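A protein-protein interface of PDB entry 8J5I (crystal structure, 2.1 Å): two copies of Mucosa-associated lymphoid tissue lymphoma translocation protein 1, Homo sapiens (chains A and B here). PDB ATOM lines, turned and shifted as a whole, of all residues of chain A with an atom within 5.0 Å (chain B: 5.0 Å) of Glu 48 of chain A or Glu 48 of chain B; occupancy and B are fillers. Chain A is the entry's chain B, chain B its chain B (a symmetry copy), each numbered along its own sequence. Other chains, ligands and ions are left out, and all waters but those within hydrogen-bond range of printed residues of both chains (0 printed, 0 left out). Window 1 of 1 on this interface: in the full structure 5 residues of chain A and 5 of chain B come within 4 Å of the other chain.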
ATOM      1  N   ARG A  28      -8.107 -16.295  14.172  1.00  0.00           N
ATOM      2  CA  ARG A  28      -8.747 -15.077  13.699  1.00  0.00           C
ATOM      3  C   ARG A  28      -7.771 -14.222  12.901  1.00  0.00           C
ATOM      4  O   ARG A  28      -8.125 -13.700  11.838  1.00  0.00           O
ATOM      5  CB  ARG A  28      -9.319 -14.291  14.879  1.00  0.00           C
ATOM      6  CG  ARG A  28     -10.621 -14.868  15.416  1.00  0.00           C
ATOM      7  CD  ARG A  28     -11.186 -13.995  16.538  1.00  0.00           C
ATOM      8  NE  ARG A  28     -12.433 -14.541  17.061  1.00  0.00           N
ATOM      9  CZ  ARG A  28     -13.595 -14.500  16.422  1.00  0.00           C
ATOM     10  NH1 ARG A  28     -13.709 -13.946  15.223  1.00  0.00           N
ATOM     11  NH2 ARG A  28     -14.671 -15.021  17.000  1.00  0.00           N
ATOM     12  N   CYS A  44     -17.323 -12.234   7.599  1.00  0.00           N
ATOM     13  CA  CYS A  44     -17.519 -12.356   9.038  1.00  0.00           C
ATOM     14  C   CYS A  44     -18.415 -13.543   9.376  1.00  0.00           C
ATOM     15  O   CYS A  44     -18.231 -14.183  10.417  1.00  0.00           O
ATOM     16  CB  CYS A  44     -18.103 -11.057   9.599  1.00  0.00           C
ATOM     17  SG  CYS A  44     -16.865  -9.782   9.972  1.00  0.00           S
ATOM     18  N   LEU A  45     -19.373 -13.868   8.502  1.00  0.00           N
ATOM     19  CA  LEU A  45     -20.279 -14.986   8.761  1.00  0.00           C
ATOM     20  C   LEU A  45     -19.536 -16.324   8.814  1.00  0.00           C
ATOM     21  O   LEU A  45     -19.806 -17.156   9.695  1.00  0.00           O
ATOM     22  CB  LEU A  45     -21.377 -15.007   7.699  1.00  0.00           C
ATOM     23  CG  LEU A  45     -22.725 -15.607   8.090  1.00  0.00           C
ATOM     24  CD1 LEU A  45     -23.219 -14.998   9.385  1.00  0.00           C
ATOM     25  CD2 LEU A  45     -23.750 -15.418   6.976  1.00  0.00           C
ATOM     26  N   ASP A  46     -18.603 -16.556   7.880  1.00  0.00           N
ATOM     27  CA  ASP A  46     -17.795 -17.778   7.918  1.00  0.00           C
ATOM     28  C   ASP A  46     -17.008 -17.876   9.220  1.00  0.00           C
ATOM     29  O   ASP A  46     -16.953 -18.941   9.865  1.00  0.00           O
ATOM     30  CB  ASP A  46     -16.815 -17.822   6.740  1.00  0.00           C
ATOM     31  CG  ASP A  46     -17.429 -17.396   5.422  1.00  0.00           C
ATOM     32  OD1 ASP A  46     -18.653 -17.557   5.223  1.00  0.00           O
ATOM     33  OD2 ASP A  46     -16.658 -16.894   4.575  1.00  0.00           O
ATOM     34  N   LEU A  47     -16.351 -16.776   9.596  1.00  0.00           N
ATOM     35  CA  LEU A  47     -15.596 -16.755  10.840  1.00  0.00           C
ATOM     36  C   LEU A  47     -16.504 -17.055  12.018  1.00  0.00           C
ATOM     37  O   LEU A  47     -16.104 -17.743  12.960  1.00  0.00           O
ATOM     38  CB  LEU A  47     -14.911 -15.398  11.023  1.00  0.00           C
ATOM     39  CG  LEU A  47     -13.870 -14.969   9.984  1.00  0.00           C
ATOM     40  CD1 LEU A  47     -12.846 -14.048  10.623  1.00  0.00           C
ATOM     41  CD2 LEU A  47     -13.194 -16.172   9.354  1.00  0.00           C
ATOM     42  N   GLU A  48     -17.737 -16.553  11.973  1.00  0.00           N
ATOM     43  CA  GLU A  48     -18.700 -16.812  13.039  1.00  0.00           C
ATOM     44  C   GLU A  48     -18.977 -18.297  13.179  1.00  0.00           C
ATOM     45  O   GLU A  48     -18.983 -18.845  14.295  1.00  0.00           O
ATOM     46  CB  GLU A  48     -19.992 -16.062  12.739  1.00  0.00           C
ATOM     47  CG  GLU A  48     -20.494 -15.263  13.874  1.00  0.00           C
ATOM     48  CD  GLU A  48     -21.753 -14.520  13.525  1.00  0.00           C
ATOM     49  OE1 GLU A  48     -22.856 -15.090  13.693  1.00  0.00           O
ATOM     50  OE2 GLU A  48     -21.628 -13.360  13.076  1.00  0.00           O
ATOM     51  N   GLN A  49     -19.261 -18.952  12.052  1.00  0.00           N
ATOM     52  CA  GLN A  49     -19.528 -20.387  12.079  1.00  0.00           C
ATOM     53  C   GLN A  49     -18.355 -21.145  12.681  1.00  0.00           C
ATOM     54  O   GLN A  49     -18.548 -22.086  13.459  1.00  0.00           O
ATOM     55  CB  GLN A  49     -19.832 -20.891  10.670  1.00  0.00           C
ATOM     56  CG  GLN A  49     -20.941 -20.110   9.978  1.00  0.00           C
ATOM     57  CD  GLN A  49     -22.136 -19.869  10.884  1.00  0.00           C
ATOM     58  OE1 GLN A  49     -22.584 -18.733  11.050  1.00  0.00           O
ATOM     59  NE2 GLN A  49     -22.675 -20.944  11.461  1.00  0.00           N
ATOM     60  N   CYS A  50     -17.127 -20.746  12.337  1.00  0.00           N
ATOM     61  CA  CYS A  50     -15.967 -21.395  12.953  1.00  0.00           C
ATOM     62  C   CYS A  50     -15.872 -21.084  14.445  1.00  0.00           C
ATOM     63  O   CYS A  50     -15.537 -21.962  15.251  1.00  0.00           O
ATOM     64  CB  CYS A  50     -14.696 -20.966  12.237  1.00  0.00           C
ATOM     65  SG  CYS A  50     -14.589 -21.648  10.576  1.00  0.00           S
ATOM     66  N   SER A  51     -16.159 -19.840  14.829  1.00  0.00           N
ATOM     67  CA  SER A  51     -16.054 -19.432  16.226  1.00  0.00           C
ATOM     68  C   SER A  51     -16.981 -20.256  17.108  1.00  0.00           C
ATOM     69  O   SER A  51     -16.623 -20.626  18.234  1.00  0.00           O
ATOM     70  CB  SER A  51     -16.377 -17.937  16.350  1.00  0.00           C
ATOM     71  OG  SER A  51     -16.448 -17.532  17.705  1.00  0.00           O
ATOM     72  N   LEU A  52     -18.174 -20.566  16.600  1.00  0.00           N
ATOM     73  CA  LEU A  52     -19.141 -21.341  17.368  1.00  0.00           C
ATOM     74  C   LEU A  52     -18.680 -22.768  17.653  1.00  0.00           C
ATOM     75  O   LEU A  52     -19.297 -23.438  18.492  1.00  0.00           O
ATOM     76  CB  LEU A  52     -20.478 -21.396  16.629  1.00  0.00           C
ATOM     77  CG  LEU A  52     -21.310 -20.123  16.520  1.00  0.00           C
ATOM     78  CD1 LEU A  52     -22.592 -20.434  15.740  1.00  0.00           C
ATOM     79  CD2 LEU A  52     -21.647 -19.544  17.892  1.00  0.00           C
ATOM     80  N   ARG B  28     -25.970  -6.495   9.197  1.00  0.00           N
ATOM     81  CA  ARG B  28     -24.640  -6.909   8.776  1.00  0.00           C
ATOM     82  C   ARG B  28     -24.126  -6.029   7.645  1.00  0.00           C
ATOM     83  O   ARG B  28     -22.964  -5.608   7.661  1.00  0.00           O
ATOM     84  CB  ARG B  28     -24.655  -8.379   8.357  1.00  0.00           C
ATOM     85  CG  ARG B  28     -24.676  -9.344   9.534  1.00  0.00           C
ATOM     86  CD  ARG B  28     -24.607 -10.795   9.055  1.00  0.00           C
ATOM     87  NE  ARG B  28     -24.629 -11.727  10.176  1.00  0.00           N
ATOM     88  CZ  ARG B  28     -23.609 -11.933  10.999  1.00  0.00           C
ATOM     89  NH1 ARG B  28     -22.462 -11.284  10.860  1.00  0.00           N
ATOM     90  NH2 ARG B  28     -23.739 -12.817  11.982  1.00  0.00           N
ATOM     91  N   CYS B  44     -14.756  -8.229  13.183  1.00  0.00           N
ATOM     92  CA  CYS B  44     -15.652  -9.378  13.158  1.00  0.00           C
ATOM     93  C   CYS B  44     -16.102  -9.760  14.565  1.00  0.00           C
ATOM     94  O   CYS B  44     -17.233 -10.222  14.749  1.00  0.00           O
ATOM     95  CB  CYS B  44     -14.968 -10.560  12.467  1.00  0.00           C
ATOM     96  SG  CYS B  44     -15.095 -10.542  10.655  1.00  0.00           S
ATOM     97  N   LEU B  45     -15.246  -9.553  15.569  1.00  0.00           N
ATOM     98  CA  LEU B  45     -15.601  -9.904  16.944  1.00  0.00           C
ATOM     99  C   LEU B  45     -16.782  -9.076  17.458  1.00  0.00           C
ATOM    100  O   LEU B  45     -17.692  -9.619  18.105  1.00  0.00           O
ATOM    101  CB  LEU B  45     -14.377  -9.736  17.843  1.00  0.00           C
ATOM    102  CG  LEU B  45     -14.294 -10.611  19.092  1.00  0.00           C
ATOM    103  CD1 LEU B  45     -14.525 -12.064  18.735  1.00  0.00           C
ATOM    104  CD2 LEU B  45     -12.953 -10.432  19.796  1.00  0.00           C
ATOM    105  N   ASP B  46     -16.787  -7.763  17.191  1.00  0.00           N
ATOM    106  CA  ASP B  46     -17.924  -6.925  17.579  1.00  0.00           C
ATOM    107  C   ASP B  46     -19.214  -7.413  16.928  1.00  0.00           C
ATOM    108  O   ASP B  46     -20.270  -7.514  17.580  1.00  0.00           O
ATOM    109  CB  ASP B  46     -17.688  -5.464  17.181  1.00  0.00           C
ATOM    110  CG  ASP B  46     -16.286  -4.972  17.478  1.00  0.00           C
ATOM    111  OD1 ASP B  46     -15.634  -5.477  18.418  1.00  0.00           O
ATOM    112  OD2 ASP B  46     -15.841  -4.057  16.750  1.00  0.00           O
ATOM    113  N   LEU B  47     -19.151  -7.675  15.620  1.00  0.00           N
ATOM    114  CA  LEU B  47     -20.318  -8.176  14.910  1.00  0.00           C
ATOM    115  C   LEU B  47     -20.790  -9.483  15.520  1.00  0.00           C
ATOM    116  O   LEU B  47     -21.994  -9.731  15.619  1.00  0.00           O
ATOM    117  CB  LEU B  47     -19.998  -8.361  13.425  1.00  0.00           C
ATOM    118  CG  LEU B  47     -19.608  -7.123  12.611  1.00  0.00           C
ATOM    119  CD1 LEU B  47     -20.004  -7.311  11.156  1.00  0.00           C
ATOM    120  CD2 LEU B  47     -20.239  -5.869  13.182  1.00  0.00           C
ATOM    121  N   GLU B  48     -19.850 -10.326  15.943  1.00  0.00           N
ATOM    122  CA  GLU B  48     -20.198 -11.594  16.575  1.00  0.00           C
ATOM    123  C   GLU B  48     -21.005 -11.373  17.840  1.00  0.00           C
ATOM    124  O   GLU B  48     -22.035 -12.032  18.066  1.00  0.00           O
ATOM    125  CB  GLU B  48     -18.921 -12.362  16.894  1.00  0.00           C
ATOM    126  CG  GLU B  48     -18.935 -13.762  16.428  1.00  0.00           C
ATOM    127  CD  GLU B  48     -17.646 -14.471  16.739  1.00  0.00           C
ATOM    128  OE1 GLU B  48     -17.527 -15.047  17.846  1.00  0.00           O
ATOM    129  OE2 GLU B  48     -16.751 -14.442  15.868  1.00  0.00           O
ATOM    130  N   GLN B  49     -20.517 -10.479  18.702  1.00  0.00           N
ATOM    131  CA  GLN B  49     -21.228 -10.185  19.943  1.00  0.00           C
ATOM    132  C   GLN B  49     -22.644  -9.709  19.655  1.00  0.00           C
ATOM    133  O   GLN B  49     -23.589 -10.094  20.352  1.00  0.00           O
ATOM    134  CB  GLN B  49     -20.461  -9.141  20.752  1.00  0.00           C
ATOM    135  CG  GLN B  49     -19.007  -9.519  20.996  1.00  0.00           C
ATOM    136  CD  GLN B  49     -18.846 -10.966  21.431  1.00  0.00           C
ATOM    137  OE1 GLN B  49     -18.071 -11.720  20.840  1.00  0.00           O
ATOM    138  NE2 GLN B  49     -19.566 -11.357  22.483  1.00  0.00           N
ATOM    139  N   CYS B  50     -22.812  -8.873  18.626  1.00  0.00           N
ATOM    140  CA  CYS B  50     -24.167  -8.452  18.263  1.00  0.00           C
ATOM    141  C   CYS B  50     -24.994  -9.615  17.719  1.00  0.00           C
ATOM    142  O   CYS B  50     -26.187  -9.737  18.024  1.00  0.00           O
ATOM    143  CB  CYS B  50     -24.101  -7.323  17.247  1.00  0.00           C
ATOM    144  SG  CYS B  50     -23.482  -5.795  17.968  1.00  0.00           S
ATOM    145  N   SER B  51     -24.378 -10.475  16.908  1.00  0.00           N
ATOM    146  CA  SER B  51     -25.091 -11.593  16.300  1.00  0.00           C
ATOM    147  C   SER B  51     -25.666 -12.518  17.363  1.00  0.00           C
ATOM    148  O   SER B  51     -26.783 -13.032  17.220  1.00  0.00           O
ATOM    149  CB  SER B  51     -24.145 -12.361  15.368  1.00  0.00           C
ATOM    150  OG  SER B  51     -24.745 -13.548  14.883  1.00  0.00           O
ATOM    151  N   LEU B  52     -24.917 -12.726  18.446  1.00  0.00           N
ATOM    152  CA  LEU B  52     -25.369 -13.605  19.517  1.00  0.00           C
ATOM    153  C   LEU B  52     -26.609 -13.084  20.241  1.00  0.00           C
ATOM    154  O   LEU B  52     -27.224 -13.849  20.997  1.00  0.00           O
ATOM    155  CB  LEU B  52     -24.253 -13.806  20.541  1.00  0.00           C
ATOM    156  CG  LEU B  52     -23.028 -14.622  20.142  1.00  0.00           C
ATOM    157  CD1 LEU B  52     -22.061 -14.676  21.329  1.00  0.00           C
ATOM    158  CD2 LEU B  52     -23.405 -16.031  19.694  1.00  0.00           C
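CD1 of Leu 45 of chain B touches NH2 of Arg 28 of chain A (3.4 Å). NH2 of Arg 28 of chain B touches CD1 of Leu 45 of chain A (3.4 Å). CG of Glu 48 of chain B touches CG of Glu 48 of chain A, at 3.3 Å.
The guanidinium group (NH2) of Arg 28 of chain A is in hydrogen-bond range of the side-chain hydroxyl (OG) of Ser 51 of chain A. The backbone carbonyl oxygen (O) of Leu 45 of chain B sits close to the side-chain amide oxygen (OE1) of Gln 49 of chain B (3.5 Å). The guanidinium group (NH2) of Arg 28 of chain B lies within hydrogen-bond range of the side-chain hydroxyl (OG) of Ser 51 of chain B. OE1 of Gln 49 of chain A lies close to O of Leu 45 of chain A (3.5 Å).
OE2 of Glu 48 of chain A lies within salt-bridge range of NH2 of Arg 28 of chain B, 2.4 Å away. OG of Ser 51 of chain A is in hydrogen-bond range of OE1 of Glu 48 of chain B. The side-chain carboxylate (OE1) of Glu 48 of chain A lies within hydrogen-bond range of the side-chain hydroxyl (OG) of Ser 51 of chain B (2.7 Å). The guanidinium group of Arg 28 of chain A lies within salt-bridge range of the side-chain carboxylate of Glu 48 of chain B (2.4 Å). The side-chain sulfur (SG) of Cys 44 of chain A forms a disulfide with the side-chain sulfur (SG) of Cys 44 of chain B, 2.0 Å away.
Arg 28 of chain A touches Leu 45 of chain B, and with the chains exchanged Leu 45 of chain A touches Arg 28 of chain B. Arg 28 of chain A touches Glu 48 of chain B, and with the chains exchanged Glu 48 of chain A touches Arg 28 of chain B. Cys 44 of chain A touches its own counterpart, Cys 44 of chain B. Glu 48 of chain A touches Ser 51 of chain B, and with the chains exchanged Ser 51 of chain A touches Glu 48 of chain B. Positions printed for both chains: 28, 44, 45, 46, 47, 48, 49, 50, 51 and 52. Of the 8 pairs that touch across the chains among the printed residues, 8 have their exchanged pair printed and touching as well.
Hydrophobic or aromatic side chains of chain A within 4 Å of the printed part of chain B: Leu 45. Among the printed residues, Asp or Glu carboxylates within 4 Å of a Lys or Arg side-chain nitrogen of the other chain: Arg 28 of chain A with Glu 48 of chain B and Glu 48 of chain A with Arg 28 of chain B.
Glu 48 of chain B touches just these residues of chain A: Arg 28 (2.4 Å), Glu 48 (3.3 Å) and Ser 51 (2.7 Å). Of the printed residues of chain A, Ser 51 of chain B touches Glu 48 (2.7 Å). Printed residues of chain B within 4 Å of Cys 44 of chain A: Cys 44. Of the printed residues of chain A, Arg 28 of chain B touches Leu 45 and Glu 48. Printed residues of chain A within 4 Å of Leu 45 of chain B: Arg 28 (3.4 Å). Of the printed residues of chain A, Cys 44 of chain B touches Cys 44. The nearest residue of chain B that does not touch Glu 48 of chain A is Leu 47 of chain B (4.4 Å).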
